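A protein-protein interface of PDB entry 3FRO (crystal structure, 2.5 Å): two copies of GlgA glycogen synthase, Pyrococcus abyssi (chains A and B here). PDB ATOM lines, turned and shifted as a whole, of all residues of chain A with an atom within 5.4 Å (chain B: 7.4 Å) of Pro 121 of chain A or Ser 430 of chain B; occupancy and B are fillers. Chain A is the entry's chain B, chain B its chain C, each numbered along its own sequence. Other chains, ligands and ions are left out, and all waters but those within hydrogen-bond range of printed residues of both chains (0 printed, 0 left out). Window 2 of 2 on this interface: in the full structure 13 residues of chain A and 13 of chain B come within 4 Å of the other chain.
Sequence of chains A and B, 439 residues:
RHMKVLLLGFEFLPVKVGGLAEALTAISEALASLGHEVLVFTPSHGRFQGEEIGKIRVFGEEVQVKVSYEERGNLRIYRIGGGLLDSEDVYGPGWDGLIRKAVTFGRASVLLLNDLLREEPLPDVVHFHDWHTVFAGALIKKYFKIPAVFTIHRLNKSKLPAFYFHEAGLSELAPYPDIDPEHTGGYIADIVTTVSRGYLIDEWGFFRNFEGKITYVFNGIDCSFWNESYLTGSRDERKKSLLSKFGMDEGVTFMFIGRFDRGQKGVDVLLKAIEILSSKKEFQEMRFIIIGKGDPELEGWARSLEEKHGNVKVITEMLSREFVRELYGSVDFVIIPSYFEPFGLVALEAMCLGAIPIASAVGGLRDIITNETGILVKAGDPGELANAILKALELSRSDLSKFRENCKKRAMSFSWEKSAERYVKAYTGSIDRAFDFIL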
ATOM      1  N   LYS A   4      -3.106  -6.632 -10.390  1.00  0.00           N
ATOM      2  CA  LYS A   4      -3.486  -7.344 -11.599  1.00  0.00           C
ATOM      3  C   LYS A   4      -3.058  -6.468 -12.774  1.00  0.00           C
ATOM      4  O   LYS A   4      -3.527  -5.334 -12.909  1.00  0.00           O
ATOM      5  CB  LYS A   4      -4.993  -7.591 -11.616  1.00  0.00           C
ATOM      6  CG  LYS A   4      -5.432  -8.760 -12.484  1.00  0.00           C
ATOM      7  CD  LYS A   4      -6.931  -8.716 -12.753  1.00  0.00           C
ATOM      8  CE  LYS A   4      -7.524 -10.098 -12.946  1.00  0.00           C
ATOM      9  NZ  LYS A   4      -7.882 -10.713 -11.642  1.00  0.00           N
ATOM     10  N   LEU A 117     -13.997 -10.521 -17.590  1.00  0.00           N
ATOM     11  CA  LEU A 117     -14.674  -9.755 -16.541  1.00  0.00           C
ATOM     12  C   LEU A 117     -16.010 -10.359 -16.117  1.00  0.00           C
ATOM     13  O   LEU A 117     -16.584  -9.956 -15.101  1.00  0.00           O
ATOM     14  CB  LEU A 117     -14.885  -8.302 -16.988  1.00  0.00           C
ATOM     15  CG  LEU A 117     -13.616  -7.458 -17.061  1.00  0.00           C
ATOM     16  CD1 LEU A 117     -13.896  -6.132 -17.749  1.00  0.00           C
ATOM     17  CD2 LEU A 117     -13.053  -7.246 -15.671  1.00  0.00           C
ATOM     18  N   GLU A 119     -16.218 -13.353 -15.108  1.00  0.00           N
ATOM     19  CA  GLU A 119     -15.888 -14.235 -13.987  1.00  0.00           C
ATOM     20  C   GLU A 119     -14.651 -13.824 -13.174  1.00  0.00           C
ATOM     21  O   GLU A 119     -14.208 -14.591 -12.319  1.00  0.00           O
ATOM     22  CB  GLU A 119     -15.710 -15.679 -14.490  1.00  0.00           C
ATOM     23  CG  GLU A 119     -16.975 -16.341 -15.059  1.00  0.00           C
ATOM     24  CD  GLU A 119     -17.976 -16.768 -13.986  1.00  0.00           C
ATOM     25  OE1 GLU A 119     -17.951 -16.211 -12.865  1.00  0.00           O
ATOM     26  OE2 GLU A 119     -18.799 -17.667 -14.270  1.00  0.00           O
ATOM     27  N   GLU A 120     -14.098 -12.632 -13.405  1.00  0.00           N
ATOM     28  CA  GLU A 120     -12.946 -12.179 -12.610  1.00  0.00           C
ATOM     29  C   GLU A 120     -12.838 -10.650 -12.472  1.00  0.00           C
ATOM     30  O   GLU A 120     -13.417  -9.910 -13.271  1.00  0.00           O
ATOM     31  CB  GLU A 120     -11.645 -12.770 -13.171  1.00  0.00           C
ATOM     32  CG  GLU A 120     -10.939 -11.935 -14.231  1.00  0.00           C
ATOM     33  CD  GLU A 120      -9.841 -12.714 -14.929  1.00  0.00           C
ATOM     34  OE1 GLU A 120      -8.653 -12.448 -14.655  1.00  0.00           O
ATOM     35  OE2 GLU A 120     -10.172 -13.608 -15.738  1.00  0.00           O
ATOM     36  N   PRO A 121     -12.091 -10.174 -11.453  1.00  0.00           N
ATOM     37  CA  PRO A 121     -11.983  -8.736 -11.210  1.00  0.00           C
ATOM     38  C   PRO A 121     -11.251  -7.978 -12.315  1.00  0.00           C
ATOM     39  O   PRO A 121     -10.474  -8.566 -13.073  1.00  0.00           O
ATOM     40  CB  PRO A 121     -11.194  -8.647  -9.892  1.00  0.00           C
ATOM     41  CG  PRO A 121     -11.237 -10.004  -9.306  1.00  0.00           C
ATOM     42  CD  PRO A 121     -11.320 -10.942 -10.459  1.00  0.00           C
ATOM     43  N   LEU A 122     -11.513  -6.677 -12.386  1.00  0.00           N
ATOM     44  CA  LEU A 122     -10.919  -5.802 -13.388  1.00  0.00           C
ATOM     45  C   LEU A 122      -9.444  -5.566 -13.064  1.00  0.00           C
ATOM     46  O   LEU A 122      -9.095  -5.386 -11.896  1.00  0.00           O
ATOM     47  CB  LEU A 122     -11.676  -4.469 -13.401  1.00  0.00           C
ATOM     48  CG  LEU A 122     -11.356  -3.413 -14.457  1.00  0.00           C
ATOM     49  CD1 LEU A 122     -11.831  -3.840 -15.834  1.00  0.00           C
ATOM     50  CD2 LEU A 122     -12.000  -2.091 -14.057  1.00  0.00           C
ATOM     51  N   PRO A 123      -8.569  -5.576 -14.087  1.00  0.00           N
ATOM     52  CA  PRO A 123      -7.157  -5.285 -13.823  1.00  0.00           C
ATOM     53  C   PRO A 123      -6.901  -3.864 -13.310  1.00  0.00           C
ATOM     54  O   PRO A 123      -7.655  -2.944 -13.626  1.00  0.00           O
ATOM     55  CB  PRO A 123      -6.476  -5.517 -15.182  1.00  0.00           C
ATOM     56  CG  PRO A 123      -7.548  -5.482 -16.183  1.00  0.00           C
ATOM     57  CD  PRO A 123      -8.815  -5.884 -15.506  1.00  0.00           C
ATOM     58  N   ARG B   1     -12.896  -8.013  -0.290  1.00  0.00           N
ATOM     59  CA  ARG B   1     -14.205  -8.731  -0.310  1.00  0.00           C
ATOM     60  C   ARG B   1     -15.380  -7.793  -0.003  1.00  0.00           C
ATOM     61  O   ARG B   1     -16.198  -7.512  -0.879  1.00  0.00           O
ATOM     62  CB  ARG B   1     -14.196  -9.901   0.692  1.00  0.00           C
ATOM     63  CG  ARG B   1     -13.574 -11.215   0.184  1.00  0.00           C
ATOM     64  CD  ARG B   1     -12.033 -11.209   0.177  1.00  0.00           C
ATOM     65  NE  ARG B   1     -11.462 -11.003  -1.159  1.00  0.00           N
ATOM     66  CZ  ARG B   1     -10.156 -11.016  -1.441  1.00  0.00           C
ATOM     67  NH1 ARG B   1      -9.251 -11.220  -0.485  1.00  0.00           N
ATOM     68  NH2 ARG B   1      -9.750 -10.821  -2.692  1.00  0.00           N
ATOM     69  N   ILE B 191     -21.205   2.890 -14.142  1.00  0.00           N
ATOM     70  CA  ILE B 191     -21.813   1.745 -14.819  1.00  0.00           C
ATOM     71  C   ILE B 191     -23.334   1.891 -14.801  1.00  0.00           C
ATOM     72  O   ILE B 191     -23.919   2.238 -13.773  1.00  0.00           O
ATOM     73  CB  ILE B 191     -21.426   0.388 -14.161  1.00  0.00           C
ATOM     74  CG1 ILE B 191     -19.999  -0.032 -14.547  1.00  0.00           C
ATOM     75  CG2 ILE B 191     -22.403  -0.715 -14.567  1.00  0.00           C
ATOM     76  CD1 ILE B 191     -18.975   0.231 -13.476  1.00  0.00           C
ATOM     77  N   GLU B 421     -24.757 -10.854  -6.141  1.00  0.00           N
ATOM     78  CA  GLU B 421     -23.345 -11.115  -6.453  1.00  0.00           C
ATOM     79  C   GLU B 421     -22.864 -10.364  -7.686  1.00  0.00           C
ATOM     80  O   GLU B 421     -21.704  -9.959  -7.760  1.00  0.00           O
ATOM     81  CB  GLU B 421     -23.117 -12.614  -6.689  1.00  0.00           C
ATOM     82  CG  GLU B 421     -23.111 -13.464  -5.432  1.00  0.00           C
ATOM     83  CD  GLU B 421     -23.173 -14.953  -5.731  1.00  0.00           C
ATOM     84  OE1 GLU B 421     -23.109 -15.336  -6.926  1.00  0.00           O
ATOM     85  OE2 GLU B 421     -23.286 -15.746  -4.769  1.00  0.00           O
ATOM     86  N   ARG B 422     -23.757 -10.194  -8.655  1.00  0.00           N
ATOM     87  CA  ARG B 422     -23.419  -9.548  -9.917  1.00  0.00           C
ATOM     88  C   ARG B 422     -23.468  -8.018  -9.828  1.00  0.00           C
ATOM     89  O   ARG B 422     -22.784  -7.327 -10.586  1.00  0.00           O
ATOM     90  CB  ARG B 422     -24.346 -10.060 -11.020  1.00  0.00           C
ATOM     91  CG  ARG B 422     -23.907  -9.679 -12.413  1.00  0.00           C
ATOM     92  CD  ARG B 422     -24.565 -10.552 -13.460  1.00  0.00           C
ATOM     93  NE  ARG B 422     -24.555  -9.902 -14.766  1.00  0.00           N
ATOM     94  CZ  ARG B 422     -23.486  -9.801 -15.553  1.00  0.00           C
ATOM     95  NH1 ARG B 422     -22.319 -10.326 -15.189  1.00  0.00           N
ATOM     96  NH2 ARG B 422     -23.586  -9.174 -16.722  1.00  0.00           N
ATOM     97  N   VAL B 424     -22.442  -6.486  -7.044  1.00  0.00           N
ATOM     98  CA  VAL B 424     -21.133  -6.275  -6.406  1.00  0.00           C
ATOM     99  C   VAL B 424     -20.024  -6.152  -7.457  1.00  0.00           C
ATOM    100  O   VAL B 424     -19.084  -5.372  -7.300  1.00  0.00           O
ATOM    101  CB  VAL B 424     -20.777  -7.408  -5.412  1.00  0.00           C
ATOM    102  CG1 VAL B 424     -19.471  -7.098  -4.703  1.00  0.00           C
ATOM    103  CG2 VAL B 424     -21.883  -7.598  -4.390  1.00  0.00           C
ATOM    104  N   LYS B 425     -20.145  -6.924  -8.532  1.00  0.00           N
ATOM    105  CA  LYS B 425     -19.242  -6.796  -9.673  1.00  0.00           C
ATOM    106  C   LYS B 425     -19.385  -5.430 -10.355  1.00  0.00           C
ATOM    107  O   LYS B 425     -18.386  -4.771 -10.650  1.00  0.00           O
ATOM    108  CB  LYS B 425     -19.490  -7.923 -10.676  1.00  0.00           C
ATOM    109  CG  LYS B 425     -18.848  -9.242 -10.283  1.00  0.00           C
ATOM    110  CD  LYS B 425     -19.123 -10.323 -11.321  1.00  0.00           C
ATOM    111  CE  LYS B 425     -17.871 -11.116 -11.650  1.00  0.00           C
ATOM    112  NZ  LYS B 425     -16.864 -10.297 -12.386  1.00  0.00           N
ATOM    113  N   ALA B 426     -20.626  -5.005 -10.593  1.00  0.00           N
ATOM    114  CA  ALA B 426     -20.893  -3.710 -11.233  1.00  0.00           C
ATOM    115  C   ALA B 426     -20.342  -2.540 -10.412  1.00  0.00           C
ATOM    116  O   ALA B 426     -19.883  -1.539 -10.973  1.00  0.00           O
ATOM    117  CB  ALA B 426     -22.391  -3.529 -11.468  1.00  0.00           C
ATOM    118  N   TYR B 427     -20.373  -2.682  -9.089  1.00  0.00           N
ATOM    119  CA  TYR B 427     -19.928  -1.629  -8.179  1.00  0.00           C
ATOM    120  C   TYR B 427     -18.449  -1.252  -8.344  1.00  0.00           C
ATOM    121  O   TYR B 427     -18.066  -0.117  -8.055  1.00  0.00           O
ATOM    122  CB  TYR B 427     -20.214  -2.021  -6.717  1.00  0.00           C
ATOM    123  CG  TYR B 427     -21.688  -2.208  -6.362  1.00  0.00           C
ATOM    124  CD1 TYR B 427     -22.063  -3.022  -5.297  1.00  0.00           C
ATOM    125  CD2 TYR B 427     -22.701  -1.574  -7.085  1.00  0.00           C
ATOM    126  CE1 TYR B 427     -23.399  -3.199  -4.959  1.00  0.00           C
ATOM    127  CE2 TYR B 427     -24.037  -1.749  -6.756  1.00  0.00           C
ATOM    128  CZ  TYR B 427     -24.380  -2.561  -5.693  1.00  0.00           C
ATOM    129  OH  TYR B 427     -25.707  -2.738  -5.372  1.00  0.00           O
ATOM    130  N   THR B 428     -17.630  -2.193  -8.812  1.00  0.00           N
ATOM    131  CA  THR B 428     -16.202  -1.946  -9.047  1.00  0.00           C
ATOM    132  C   THR B 428     -15.829  -1.950 -10.536  1.00  0.00           C
ATOM    133  O   THR B 428     -14.652  -1.830 -10.886  1.00  0.00           O
ATOM    134  CB  THR B 428     -15.343  -3.009  -8.338  1.00  0.00           C
ATOM    135  OG1 THR B 428     -15.643  -4.302  -8.878  1.00  0.00           O
ATOM    136  CG2 THR B 428     -15.608  -2.998  -6.831  1.00  0.00           C
ATOM    137  N   GLY B 429     -16.824  -2.089 -11.408  1.00  0.00           N
ATOM    138  CA  GLY B 429     -16.578  -2.182 -12.846  1.00  0.00           C
ATOM    139  C   GLY B 429     -16.036  -3.531 -13.294  1.00  0.00           C
ATOM    140  O   GLY B 429     -15.637  -3.693 -14.448  1.00  0.00           O
ATOM    141  N   SER B 430     -16.036  -4.507 -12.390  1.00  0.00           N
ATOM    142  CA  SER B 430     -15.534  -5.842 -12.689  1.00  0.00           C
ATOM    143  C   SER B 430     -16.651  -6.666 -13.308  1.00  0.00           C
ATOM    144  O   SER B 430     -17.034  -7.705 -12.781  1.00  0.00           O
ATOM    145  CB  SER B 430     -15.020  -6.514 -11.417  1.00  0.00           C
ATOM    146  OG  SER B 430     -13.845  -5.880 -10.959  1.00  0.00           O
ATOM    147  N   ILE B 431     -17.162  -6.192 -14.440  1.00  0.00           N
ATOM    148  CA  ILE B 431     -18.330  -6.781 -15.072  1.00  0.00           C
ATOM    149  C   ILE B 431     -18.261  -6.559 -16.579  1.00  0.00           C
ATOM    150  O   ILE B 431     -17.630  -5.613 -17.042  1.00  0.00           O
ATOM    151  CB  ILE B 431     -19.624  -6.165 -14.490  1.00  0.00           C
ATOM    152  CG1 ILE B 431     -20.854  -6.964 -14.919  1.00  0.00           C
ATOM    153  CG2 ILE B 431     -19.757  -4.699 -14.895  1.00  0.00           C
ATOM    154  CD1 ILE B 431     -22.068  -6.694 -14.065  1.00  0.00           C
ATOM    155  N   ASP B 432     -18.894  -7.446 -17.340  1.00  0.00           N
ATOM    156  CA  ASP B 432     -18.988  -7.287 -18.792  1.00  0.00           C
ATOM    157  C   ASP B 432     -20.063  -6.264 -19.148  1.00  0.00           C
ATOM    158  O   ASP B 432     -20.918  -5.937 -18.325  1.00  0.00           O
ATOM    159  CB  ASP B 432     -19.301  -8.622 -19.470  1.00  0.00           C
ATOM    160  CG  ASP B 432     -20.601  -9.227 -18.989  1.00  0.00           C
ATOM    161  OD1 ASP B 432     -20.671  -9.602 -17.800  1.00  0.00           O
ATOM    162  OD2 ASP B 432     -21.549  -9.331 -19.798  1.00  0.00           O
ATOM    163  N   ARG B 433     -20.023  -5.775 -20.384  1.00  0.00           N
ATOM    164  CA  ARG B 433     -20.943  -4.730 -20.839  1.00  0.00           C
ATOM    165  C   ARG B 433     -21.241  -4.864 -22.332  1.00  0.00           C
ATOM    166  O   ARG B 433     -20.580  -5.625 -23.042  1.00  0.00           O
ATOM    167  CB  ARG B 433     -20.379  -3.337 -20.521  1.00  0.00           C
ATOM    168  CG  ARG B 433     -18.857  -3.248 -20.601  1.00  0.00           C
ATOM    169  CD  ARG B 433     -18.183  -3.292 -19.229  1.00  0.00           C
ATOM    170  NE  ARG B 433     -17.456  -2.057 -18.971  1.00  0.00           N
ATOM    171  CZ  ARG B 433     -16.946  -1.706 -17.795  1.00  0.00           C
ATOM    172  NH1 ARG B 433     -17.055  -2.490 -16.733  1.00  0.00           N
ATOM    173  NH2 ARG B 433     -16.311  -0.552 -17.685  1.00  0.00           N
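NZ of Lys 425 of chain B sits at hydrogen-bond distance from O of Leu 117 of chain A (2.8 Å). OG of Ser 430 of chain B sits at hydrogen-bond distance from N of Leu 122 of chain A (2.8 Å). The backbone carbonyl oxygen (O) of Leu 117 of chain A sits close to the backbone carbonyl oxygen (O) of Ser 430 of chain B.
NZ of Lys 4 of chain A is in salt-bridge range of OE1 of Glu 120 of chain A (3.6 Å). The backbone carbonyl oxygen (O) of Lys 425 of chain B sits at hydrogen-bond distance from the side-chain hydroxyl (OG1) of Thr 428 of chain B (3.3 Å). The side-chain amino group (NZ) of Lys 425 of chain B sits at hydrogen-bond distance from the backbone carbonyl oxygen (O) of Ser 430 of chain B, at 2.6 Å. The side-chain hydroxyl of Ser 430 of chain B lies within hydrogen-bond range of the side-chain hydroxyl of Thr 428 of chain B. NH1 of Arg 433 of chain B lies within hydrogen-bond range of O of Gly 429 of chain B, 2.9 Å away. NH1 of Arg 433 of chain B sits at hydrogen-bond distance from O of Ile 431 of chain B (3.2 Å).
CA of Ile 431 of chain B touches O of Leu 117 of chain A, 3.6 Å away. Lys 425 of chain B touches Glu 120 of chain A (NZ to O, 3.6 Å). CA of Pro 121 of chain A touches OG of Ser 430 of chain B, at 3.4 Å. Leu 122 of chain A touches Gly 429 of chain B.
Of the printed residues of chain B, Pro 121 of chain A touches Ser 430 (3.4 Å). Ser 430 of chain B touches just these residues of chain A: Leu 117 (3.3 Å), Pro 121 (3.4 Å) and Leu 122 (2.8 Å). Of the printed residues of chain B, Glu 120 of chain A touches Lys 425 (3.6 Å). Of the printed residues of chain A, Gly 429 of chain B touches Leu 122. Tyr 427 of chain B touches none of the printed residues of chain A. Arg 1 of chain B touches none of the printed residues of chain A. The nearest residue of chain B that does not touch Pro 121 of chain A is Lys 425 of chain B (4.9 Å). The nearest printed residue of chain A that does not touch Gly 429 of chain B is Leu 117 of chain A (4.5 Å).
Printed residues of chain A that touch a printed residue of chain B: Leu 117, Glu 120, Pro 121 and Leu 122. Hydrophobic or aromatic side chains of chain A that line the printed part of chain B: Leu 117, Pro 121 and Leu 122. Of the 14 printed residues of chain B, 4 touch a printed residue of chain A. Among the printed residues, 7 pairs touch across the chains.
No position is printed for both chains. Of the 7 pairs that touch across the chains among the printed residues, none has its exchanged pair printed and touching as well.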
